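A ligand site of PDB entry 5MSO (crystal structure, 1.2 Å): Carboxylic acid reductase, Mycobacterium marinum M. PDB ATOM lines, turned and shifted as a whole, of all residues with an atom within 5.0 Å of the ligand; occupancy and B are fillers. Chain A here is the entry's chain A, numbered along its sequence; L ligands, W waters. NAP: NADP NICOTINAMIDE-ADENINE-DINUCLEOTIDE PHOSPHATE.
N of Cys 983 lies within hydrogen-bond range of O of Ser 920 (3.0 Å).
The side-chain amino group (NZ) of Lys 855 sits at hydrogen-bond distance from the backbone carbonyl oxygen (O) of Ala 881 (2.8 Å).
O of Thr 919 lies within hydrogen-bond range of NZ of Lys 960 (2.8 Å).
The backbone carbonyl oxygen (O) of Arg 814 lies within hydrogen-bond range of the guanidinium group (NH1) of Arg 824 (2.9 Å).
N of Gly 856 sits at hydrogen-bond distance from OD1 of Asp 854, at 3.0 Å.
The side-chain hydroxyl of Tyr 956 sits at hydrogen-bond distance from an oxygen (O2D) of the ligand, 2.7 Å away.
An oxygen (O3D) of the ligand lies within hydrogen-bond range of the side-chain hydroxyl of Thr 919 (2.8 Å).
The backbone NH of Lys 855 lies within hydrogen-bond range of a nitrogen (N1A) of the ligand (3.0 Å).
The backbone NH (N) of Phe 789 sits at hydrogen-bond distance from an oxygen (O1A) of the ligand, 2.8 Å away.
The side-chain amino group (NZ) of Lys 960 sits at hydrogen-bond distance from an oxygen (O3D) of the ligand (3.0 Å).
O of Pro 880 sits at hydrogen-bond distance from O3D of the ligand.
The guanidinium group (NH2) of Arg 824 lies within salt-bridge range of an oxygen (O2X) of the ligand.
OD1 of Asp 854 lies within hydrogen-bond range of N6A of the ligand, 2.9 Å away.
An oxygen (O2X) of the ligand lies within hydrogen-bond range of the side-chain hydroxyl (OG1) of Thr 787 (2.7 Å).
The backbone NH (N) of Leu 790 lies within hydrogen-bond range of an oxygen (O1N) of the ligand.
N of Ala 882 is in hydrogen-bond range of O4B of the ligand, 3.2 Å away.
N of Gly 788 lies within hydrogen-bond range of O3B of the ligand, 3.1 Å away.
An oxygen (O3B) of the ligand sits close to the backbone carbonyl oxygen (O) of Gly 785 (3.3 Å).
O2N of the ligand sits at hydrogen-bond distance from N of Gly 791 (3.0 Å).
NH2 of Arg 814 is in salt-bridge range of O1X of the ligand.
Water W7 bridges O1N of the ligand (2.7 Å) and ND2 of Asn 997 (3.4 Å).
Water W2 lies within hydrogen-bond range of an oxygen (O2A) of the ligand, the backbone NH of Val 884 and the backbone carbonyl oxygen of Ala 882.
Water W15 lies within hydrogen-bond range of an oxygen (O2A) of the ligand (2.9 Å) and the side-chain amide nitrogen (ND2) of Asn 997 (3.2 Å).
Water W1 lies within hydrogen-bond range of O2B of the ligand (3.0 Å), N of Arg 814 (3.0 Å) and OG1 of Thr 787 (3.2 Å).
Water W12 lies within hydrogen-bond range of OH of Tyr 956 (2.8 Å), OG1 of Thr 921 (2.9 Å) and N1N of the ligand (3.2 Å).
Water W8 lies within hydrogen-bond range of O of Pro 896, NZ of Lys 855 and O of Ala 881.
O of Ser 920 lies close to N1N of the ligand (2.8 Å).
Merely in contact with the ligand: Ala 881, Val 884, Pro 896 and Cys 983.
Hydrophobic or aromatic side chains that line the ligand: Phe 789, Leu 790, Ala 881, Ala 882, Val 884, Pro 896 and Tyr 956.
Of the 28 residues printed, 20 come within 4 Å of the ligand.
The nearest printed residue that does not touch the ligand is Ala 786 (4.1 Å).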
ATOM      1  N   GLY A 785      10.259  -2.651  21.720  1.00  0.00           N
ATOM      2  CA  GLY A 785      11.109  -1.793  22.544  1.00  0.00           C
ATOM      3  C   GLY A 785      10.551  -1.194  23.796  1.00  0.00           C
ATOM      4  O   GLY A 785      11.029  -0.188  24.213  1.00  0.00           O
ATOM      5  N   ALA A 786       9.543  -1.825  24.398  1.00  0.00           N
ATOM      6  CA  ALA A 786       8.905  -1.273  25.586  1.00  0.00           C
ATOM      7  C   ALA A 786       9.818  -1.138  26.804  1.00  0.00           C
ATOM      8  O   ALA A 786       9.526  -0.361  27.662  1.00  0.00           O
ATOM      9  CB  ALA A 786       7.616  -2.014  25.940  1.00  0.00           C
ATOM     10  N   THR A 787      10.882  -1.927  26.857  1.00  0.00           N
ATOM     11  CA  THR A 787      11.862  -1.818  27.919  1.00  0.00           C
ATOM     12  C   THR A 787      12.852  -0.623  27.689  1.00  0.00           C
ATOM     13  O   THR A 787      13.564  -0.234  28.575  1.00  0.00           O
ATOM     14  CB  THR A 787      12.667  -3.104  28.106  1.00  0.00           C
ATOM     15  OG1 THR A 787      13.123  -3.534  26.833  1.00  0.00           O
ATOM     16  CG2 THR A 787      11.801  -4.172  28.759  1.00  0.00           C
ATOM     17  N   GLY A 788      12.835  -0.067  26.477  1.00  0.00           N
ATOM     18  CA  GLY A 788      13.709   1.042  26.099  1.00  0.00           C
ATOM     19  C   GLY A 788      13.264   2.340  26.724  1.00  0.00           C
ATOM     20  O   GLY A 788      12.239   2.404  27.325  1.00  0.00           O
ATOM     21  N   PHE A 789      14.079   3.379  26.581  1.00  0.00           N
ATOM     22  CA  PHE A 789      13.717   4.665  27.194  1.00  0.00           C
ATOM     23  C   PHE A 789      12.511   5.341  26.513  1.00  0.00           C
ATOM     24  O   PHE A 789      11.519   5.553  27.121  1.00  0.00           O
ATOM     25  CB  PHE A 789      14.929   5.613  27.251  1.00  0.00           C
ATOM     26  CG  PHE A 789      14.666   6.841  28.106  1.00  0.00           C
ATOM     27  CD1 PHE A 789      14.430   6.705  29.470  1.00  0.00           C
ATOM     28  CD2 PHE A 789      14.580   8.070  27.538  1.00  0.00           C
ATOM     29  CE1 PHE A 789      14.140   7.780  30.240  1.00  0.00           C
ATOM     30  CE2 PHE A 789      14.278   9.169  28.335  1.00  0.00           C
ATOM     31  CZ  PHE A 789      14.061   8.999  29.666  1.00  0.00           C
ATOM     32  N   LEU A 790      12.613   5.614  25.214  1.00  0.00           N
ATOM     33  CA  LEU A 790      11.463   6.115  24.484  1.00  0.00           C
ATOM     34  C   LEU A 790      10.355   5.030  24.493  1.00  0.00           C
ATOM     35  O   LEU A 790       9.221   5.348  24.652  1.00  0.00           O
ATOM     36  CB  LEU A 790      11.822   6.464  23.024  1.00  0.00           C
ATOM     37  CG  LEU A 790      10.633   6.819  22.112  1.00  0.00           C
ATOM     38  CD1 LEU A 790       9.861   8.007  22.646  1.00  0.00           C
ATOM     39  CD2 LEU A 790      11.137   7.061  20.703  1.00  0.00           C
ATOM     40  N   GLY A 791      10.734   3.773  24.332  1.00  0.00           N
ATOM     41  CA  GLY A 791       9.742   2.699  24.244  1.00  0.00           C
ATOM     42  C   GLY A 791       8.818   2.584  25.449  1.00  0.00           C
ATOM     43  O   GLY A 791       7.655   2.358  25.288  1.00  0.00           O
ATOM     44  N   LEU A 812       6.498  -6.884  22.469  1.00  0.00           N
ATOM     45  CA  LEU A 812       7.516  -7.872  22.158  1.00  0.00           C
ATOM     46  C   LEU A 812       8.753  -7.482  22.974  1.00  0.00           C
ATOM     47  O   LEU A 812       9.277  -6.432  22.809  1.00  0.00           O
ATOM     48  CB  LEU A 812       7.844  -7.833  20.668  1.00  0.00           C
ATOM     49  CG  LEU A 812       8.853  -8.890  20.196  1.00  0.00           C
ATOM     50  CD1 LEU A 812       8.137 -10.226  20.072  1.00  0.00           C
ATOM     51  CD2 LEU A 812       9.524  -8.493  18.902  1.00  0.00           C
ATOM     52  N   ARG A 814      12.577  -8.959  24.762  1.00  0.00           N
ATOM     53  CA  ARG A 814      13.602 -10.013  24.767  1.00  0.00           C
ATOM     54  C   ARG A 814      13.717 -10.639  26.163  1.00  0.00           C
ATOM     55  O   ARG A 814      13.901  -9.975  27.129  1.00  0.00           O
ATOM     56  CB  ARG A 814      14.982  -9.470  24.362  1.00  0.00           C
ATOM     57  CG  ARG A 814      15.049  -8.951  22.924  1.00  0.00           C
ATOM     58  CD  ARG A 814      16.483  -8.741  22.481  1.00  0.00           C
ATOM     59  NE  ARG A 814      17.145  -7.660  23.154  1.00  0.00           N
ATOM     60  CZ  ARG A 814      18.385  -7.297  22.879  1.00  0.00           C
ATOM     61  NH1 ARG A 814      19.052  -7.970  21.978  1.00  0.00           N
ATOM     62  NH2 ARG A 814      18.953  -6.311  23.529  1.00  0.00           N
ATOM     63  N   ARG A 824      10.408  -8.339  33.188  1.00  0.00           N
ATOM     64  CA  ARG A 824      11.292  -7.254  32.784  1.00  0.00           C
ATOM     65  C   ARG A 824      10.500  -5.965  32.592  1.00  0.00           C
ATOM     66  O   ARG A 824      10.926  -4.937  32.980  1.00  0.00           O
ATOM     67  CB  ARG A 824      12.014  -7.555  31.475  1.00  0.00           C
ATOM     68  CG  ARG A 824      13.044  -8.629  31.530  1.00  0.00           C
ATOM     69  CD  ARG A 824      13.889  -8.633  30.268  1.00  0.00           C
ATOM     70  NE  ARG A 824      14.632  -7.398  30.140  1.00  0.00           N
ATOM     71  CZ  ARG A 824      14.923  -6.761  29.010  1.00  0.00           C
ATOM     72  NH1 ARG A 824      14.556  -7.266  27.842  1.00  0.00           N
ATOM     73  NH2 ARG A 824      15.581  -5.637  29.061  1.00  0.00           N
ATOM     74  N   GLY A 853      10.400 -12.461  22.522  1.00  0.00           N
ATOM     75  CA  GLY A 853      10.759 -12.573  21.129  1.00  0.00           C
ATOM     76  C   GLY A 853      11.959 -11.724  20.798  1.00  0.00           C
ATOM     77  O   GLY A 853      12.542 -11.130  21.667  1.00  0.00           O
ATOM     78  N   ASP A 854      12.322 -11.711  19.535  1.00  0.00           N
ATOM     79  CA  ASP A 854      13.495 -11.020  19.052  1.00  0.00           C
ATOM     80  C   ASP A 854      13.239 -10.679  17.589  1.00  0.00           C
ATOM     81  O   ASP A 854      13.006 -11.551  16.804  1.00  0.00           O
ATOM     82  CB  ASP A 854      14.689 -11.982  19.166  1.00  0.00           C
ATOM     83  CG  ASP A 854      16.012 -11.364  18.839  1.00  0.00           C
ATOM     84  OD1 ASP A 854      16.145 -10.571  17.943  1.00  0.00           O
ATOM     85  OD2 ASP A 854      16.964 -11.736  19.486  1.00  0.00           O
ATOM     86  N   LYS A 855      13.380  -9.413  17.245  1.00  0.00           N
ATOM     87  CA  LYS A 855      13.142  -8.931  15.872  1.00  0.00           C
ATOM     88  C   LYS A 855      14.012  -9.537  14.826  1.00  0.00           C
ATOM     89  O   LYS A 855      13.638  -9.639  13.717  1.00  0.00           O
ATOM     90  CB  LYS A 855      13.310  -7.405  15.810  1.00  0.00           C
ATOM     91  CG  LYS A 855      12.140  -6.661  16.410  1.00  0.00           C
ATOM     92  CD  LYS A 855      12.448  -5.170  16.541  1.00  0.00           C
ATOM     93  CE  LYS A 855      12.869  -4.537  15.231  1.00  0.00           C
ATOM     94  NZ  LYS A 855      13.085  -3.083  15.361  1.00  0.00           N
ATOM     95  N   GLY A 856      15.204  -9.923  15.205  1.00  0.00           N
ATOM     96  CA  GLY A 856      16.134 -10.526  14.294  1.00  0.00           C
ATOM     97  C   GLY A 856      15.852 -11.945  13.876  1.00  0.00           C
ATOM     98  O   GLY A 856      16.424 -12.459  12.946  1.00  0.00           O
ATOM     99  N   PRO A 880       9.907   1.297  17.839  1.00  0.00           N
ATOM    100  CA  PRO A 880      11.082   2.061  18.265  1.00  0.00           C
ATOM    101  C   PRO A 880      12.277   1.150  18.615  1.00  0.00           C
ATOM    102  O   PRO A 880      13.328   1.650  18.810  1.00  0.00           O
ATOM    103  CB  PRO A 880      10.614   2.755  19.547  1.00  0.00           C
ATOM    104  CG  PRO A 880       9.666   1.754  20.174  1.00  0.00           C
ATOM    105  CD  PRO A 880       8.963   1.086  18.971  1.00  0.00           C
ATOM    106  N   ALA A 881      12.107  -0.163  18.683  1.00  0.00           N
ATOM    107  CA  ALA A 881      13.204  -1.037  19.080  1.00  0.00           C
ATOM    108  C   ALA A 881      14.347  -0.993  18.102  1.00  0.00           C
ATOM    109  O   ALA A 881      14.161  -0.972  16.927  1.00  0.00           O
ATOM    110  CB  ALA A 881      12.699  -2.451  19.156  1.00  0.00           C
ATOM    111  N   ALA A 882      15.540  -0.960  18.647  1.00  0.00           N
ATOM    112  CA  ALA A 882      16.767  -0.965  17.867  1.00  0.00           C
ATOM    113  C   ALA A 882      17.956  -1.167  18.802  1.00  0.00           C
ATOM    114  O   ALA A 882      17.845  -0.912  19.956  1.00  0.00           O
ATOM    115  CB  ALA A 882      16.954   0.383  17.166  1.00  0.00           C
ATOM    116  N   LEU A 883      19.071  -1.573  18.217  1.00  0.00           N
ATOM    117  CA  LEU A 883      20.329  -1.588  18.949  1.00  0.00           C
ATOM    118  C   LEU A 883      20.945  -0.193  18.650  1.00  0.00           C
ATOM    119  O   LEU A 883      21.377   0.043  17.545  1.00  0.00           O
ATOM    120  CB  LEU A 883      21.214  -2.698  18.437  1.00  0.00           C
ATOM    121  CG  LEU A 883      22.603  -2.786  19.108  1.00  0.00           C
ATOM    122  CD1 LEU A 883      22.573  -2.606  20.596  1.00  0.00           C
ATOM    123  CD2 LEU A 883      23.307  -4.066  18.726  1.00  0.00           C
ATOM    124  N   VAL A 884      20.891   0.715  19.617  1.00  0.00           N
ATOM    125  CA  VAL A 884      21.385   2.081  19.482  1.00  0.00           C
ATOM    126  C   VAL A 884      22.804   2.117  20.002  1.00  0.00           C
ATOM    127  O   VAL A 884      23.037   2.266  21.167  1.00  0.00           O
ATOM    128  CB  VAL A 884      20.533   3.089  20.259  1.00  0.00           C
ATOM    129  CG1 VAL A 884      20.971   4.505  19.987  1.00  0.00           C
ATOM    130  CG2 VAL A 884      19.060   2.928  19.913  1.00  0.00           C
ATOM    131  N   PRO A 896      19.323  -6.733  14.086  1.00  0.00           N
ATOM    132  CA  PRO A 896      18.267  -6.116  14.883  1.00  0.00           C
ATOM    133  C   PRO A 896      17.530  -4.949  14.216  1.00  0.00           C
ATOM    134  O   PRO A 896      16.376  -4.777  14.454  1.00  0.00           O
ATOM    135  CB  PRO A 896      18.985  -5.623  16.140  1.00  0.00           C
ATOM    136  CG  PRO A 896      20.408  -5.489  15.753  1.00  0.00           C
ATOM    137  CD  PRO A 896      20.627  -6.597  14.776  1.00  0.00           C
ATOM    138  N   THR A 919      10.674   4.648  14.289  1.00  0.00           N
ATOM    139  CA  THR A 919      11.595   5.694  14.672  1.00  0.00           C
ATOM    140  C   THR A 919      12.940   5.445  13.939  1.00  0.00           C
ATOM    141  O   THR A 919      13.460   4.370  13.944  1.00  0.00           O
ATOM    142  CB  THR A 919      11.827   5.782  16.184  1.00  0.00           C
ATOM    143  OG1 THR A 919      12.283   4.521  16.681  1.00  0.00           O
ATOM    144  CG2 THR A 919      10.580   6.148  16.894  1.00  0.00           C
ATOM    145  N   SER A 920      13.427   6.491  13.320  1.00  0.00           N
ATOM    146  CA  SER A 920      14.716   6.481  12.631  1.00  0.00           C
ATOM    147  C   SER A 920      15.623   7.498  13.384  1.00  0.00           C
ATOM    148  O   SER A 920      15.328   7.947  14.447  1.00  0.00           O
ATOM    149  CB  SER A 920      14.547   6.808  11.147  1.00  0.00           C
ATOM    150  OG  SER A 920      15.755   6.638  10.459  1.00  0.00           O
ATOM    151  N   THR A 921      16.746   7.809  12.776  1.00  0.00           N
ATOM    152  CA  THR A 921      17.689   8.759  13.325  1.00  0.00           C
ATOM    153  C   THR A 921      17.958   9.904  12.364  1.00  0.00           C
ATOM    154  O   THR A 921      18.046   9.703  11.194  1.00  0.00           O
ATOM    155  CB  THR A 921      19.029   8.067  13.716  1.00  0.00           C
ATOM    156  OG1 THR A 921      19.929   9.024  14.252  1.00  0.00           O
ATOM    157  CG2 THR A 921      19.731   7.365  12.539  1.00  0.00           C
ATOM    158  N   TYR A 956      25.397   2.581  12.756  1.00  0.00           N
ATOM    159  CA  TYR A 956      24.068   2.803  13.294  1.00  0.00           C
ATOM    160  C   TYR A 956      23.203   3.585  12.289  1.00  0.00           C
ATOM    161  O   TYR A 956      22.121   3.195  12.001  1.00  0.00           O
ATOM    162  CB  TYR A 956      24.193   3.586  14.585  1.00  0.00           C
ATOM    163  CG  TYR A 956      22.876   4.140  15.129  1.00  0.00           C
ATOM    164  CD1 TYR A 956      21.882   3.301  15.583  1.00  0.00           C
ATOM    165  CD2 TYR A 956      22.672   5.485  15.185  1.00  0.00           C
ATOM    166  CE1 TYR A 956      20.699   3.822  16.054  1.00  0.00           C
ATOM    167  CE2 TYR A 956      21.490   6.002  15.680  1.00  0.00           C
ATOM    168  CZ  TYR A 956      20.524   5.145  16.116  1.00  0.00           C
ATOM    169  OH  TYR A 956      19.349   5.670  16.592  1.00  0.00           O
ATOM    170  N   LYS A 960      19.669   2.291  10.353  1.00  0.00           N
ATOM    171  CA  LYS A 960      18.382   2.985  10.436  1.00  0.00           C
ATOM    172  C   LYS A 960      17.863   3.372   9.031  1.00  0.00           C
ATOM    173  O   LYS A 960      16.707   3.273   8.762  1.00  0.00           O
ATOM    174  CB  LYS A 960      18.430   4.162  11.395  1.00  0.00           C
ATOM    175  CG  LYS A 960      18.802   3.751  12.824  1.00  0.00           C
ATOM    176  CD  LYS A 960      17.820   2.772  13.499  1.00  0.00           C
ATOM    177  CE  LYS A 960      16.433   3.372  13.614  1.00  0.00           C
ATOM    178  NZ  LYS A 960      15.585   2.584  14.554  1.00  0.00           N
ATOM    179  N   CYS A 983      14.580  10.837  14.931  1.00  0.00           N
ATOM    180  CA  CYS A 983      14.890  11.380  16.248  1.00  0.00           C
ATOM    181  C   CYS A 983      16.393  11.533  16.474  1.00  0.00           C
ATOM    182  O   CYS A 983      17.210  11.058  15.709  1.00  0.00           O
ATOM    183  CB  CYS A 983      14.297  10.458  17.325  1.00  0.00           C
ATOM    184  SG  CYS A 983      12.489  10.236  17.212  1.00  0.00           S
ATOM    185  N   ILE A 986      16.990  12.505  23.062  1.00  0.00           N
ATOM    186  CA  ILE A 986      15.771  12.292  23.805  1.00  0.00           C
ATOM    187  C   ILE A 986      16.079  12.509  25.281  1.00  0.00           C
ATOM    188  O   ILE A 986      16.792  11.789  25.891  1.00  0.00           O
ATOM    189  CB  ILE A 986      15.191  10.879  23.543  1.00  0.00           C
ATOM    190  CG1 ILE A 986      14.942  10.704  22.039  1.00  0.00           C
ATOM    191  CG2 ILE A 986      13.915  10.656  24.359  1.00  0.00           C
ATOM    192  CD1 ILE A 986      14.372   9.372  21.652  1.00  0.00           C
ATOM    193  N   ASN A 997      17.765   7.480  31.026  1.00  0.00           N
ATOM    194  CA  ASN A 997      18.538   6.589  30.152  1.00  0.00           C
ATOM    195  C   ASN A 997      19.975   6.852  30.676  1.00  0.00           C
ATOM    196  O   ASN A 997      20.650   7.721  30.218  1.00  0.00           O
ATOM    197  CB  ASN A 997      18.375   7.033  28.708  1.00  0.00           C
ATOM    198  CG  ASN A 997      18.888   6.022  27.713  1.00  0.00           C
ATOM    199  OD1 ASN A 997      19.434   5.062  28.066  1.00  0.00           O
ATOM    200  ND2 ASN A 997      18.695   6.293  26.482  1.00  0.00           N
HETATM  201  PA  NAP L   1      16.734   2.211  23.888  1.00  0.00           P
HETATM  202  O1A NAP L   1      16.435   2.816  25.234  1.00  0.00           O
HETATM  203  O2A NAP L   1      18.129   2.019  23.452  1.00  0.00           O
HETATM  204  O5B NAP L   1      15.955   0.834  23.800  1.00  0.00           O
HETATM  205  C5B NAP L   1      16.137  -0.086  22.709  1.00  0.00           C
HETATM  206  C4B NAP L   1      14.985  -1.080  22.802  1.00  0.00           C
HETATM  207  O4B NAP L   1      15.065  -1.967  21.654  1.00  0.00           O
HETATM  208  C3B NAP L   1      15.014  -1.937  24.031  1.00  0.00           C
HETATM  209  O3B NAP L   1      13.645  -2.232  24.390  1.00  0.00           O
HETATM  210  C2B NAP L   1      15.681  -3.200  23.479  1.00  0.00           C
HETATM  211  O2B NAP L   1      15.434  -4.377  24.215  1.00  0.00           O
HETATM  212  C1B NAP L   1      15.010  -3.292  22.105  1.00  0.00           C
HETATM  213  N9A NAP L   1      15.708  -4.163  21.178  1.00  0.00           N
HETATM  214  C8A NAP L   1      17.021  -4.086  20.814  1.00  0.00           C
HETATM  215  N7A NAP L   1      17.341  -5.101  19.988  1.00  0.00           N
HETATM  216  C5A NAP L   1      16.210  -5.870  19.872  1.00  0.00           C
HETATM  217  C6A NAP L   1      15.898  -7.097  19.206  1.00  0.00           C
HETATM  218  N6A NAP L   1      16.813  -7.758  18.484  1.00  0.00           N
HETATM  219  N1A NAP L   1      14.620  -7.544  19.295  1.00  0.00           N
HETATM  220  C2A NAP L   1      13.696  -6.913  20.036  1.00  0.00           C
HETATM  221  N3A NAP L   1      13.913  -5.781  20.725  1.00  0.00           N
HETATM  222  C4A NAP L   1      15.153  -5.279  20.646  1.00  0.00           C
HETATM  223  O3  NAP L   1      15.976   3.106  22.728  1.00  0.00           O
HETATM  224  PN  NAP L   1      14.595   3.958  22.874  1.00  0.00           P
HETATM  225  O1N NAP L   1      14.908   5.216  23.583  1.00  0.00           O
HETATM  226  O2N NAP L   1      13.519   3.116  23.420  1.00  0.00           O
HETATM  227  O5D NAP L   1      14.283   4.199  21.318  1.00  0.00           O
HETATM  228  C5D NAP L   1      14.912   5.248  20.583  1.00  0.00           C
HETATM  229  C4D NAP L   1      14.535   5.014  19.116  1.00  0.00           C
HETATM  230  O4D NAP L   1      14.783   6.272  18.409  1.00  0.00           O
HETATM  231  C3D NAP L   1      15.396   3.990  18.402  1.00  0.00           C
HETATM  232  O3D NAP L   1      14.737   3.297  17.316  1.00  0.00           O
HETATM  233  C2D NAP L   1      16.460   4.857  17.745  1.00  0.00           C
HETATM  234  O2D NAP L   1      17.152   4.142  16.712  1.00  0.00           O
HETATM  235  C1D NAP L   1      15.636   6.036  17.282  1.00  0.00           C
HETATM  236  N1N NAP L   1      16.327   7.207  16.982  1.00  0.00           N
HETATM  237  P2B NAP L   1      16.344  -4.776  25.514  1.00  0.00           P
HETATM  238  O1X NAP L   1      17.752  -4.365  25.202  1.00  0.00           O
HETATM  239  O2X NAP L   1      15.754  -4.022  26.691  1.00  0.00           O
HETATM  240  O3X NAP L   1      16.148  -6.267  25.581  1.00  0.00           O
HETATM  241  O   HOH W   1      13.007  -5.993  24.753  1.00  0.00           O
HETATM  242  O   HOH W   2      19.709   0.136  22.220  1.00  0.00           O
HETATM  243  O   HOH W   3      12.750   1.120  21.704  1.00  0.00           O
HETATM  244  O   HOH W   4      16.544  -1.602  27.658  1.00  0.00           O
HETATM  245  O   HOH W   5      19.860  -8.415  18.216  1.00  0.00           O
HETATM  246  O   HOH W   6      13.164   1.186  15.354  1.00  0.00           O
HETATM  247  O   HOH W   7      17.188   6.578  23.428  1.00  0.00           O
HETATM  248  O   HOH W   8      15.528  -4.080  17.046  1.00  0.00           O
HETATM  249  O   HOH W   9      20.066  -5.904  19.646  1.00  0.00           O
HETATM  250  O   HOH W  10      18.026  -7.869  26.854  1.00  0.00           O
HETATM  251  O   HOH W  11      17.357   8.928  18.905  1.00  0.00           O
HETATM  252  O   HOH W  12      19.285   8.446  17.011  1.00  0.00           O
HETATM  253  O   HOH W  13      11.187  -5.331  21.194  1.00  0.00           O
HETATM  254  O   HOH W  14      17.892   2.582  27.470  1.00  0.00           O
HETATM  255  O   HOH W  15      19.297   4.693  23.751  1.00  0.00           O
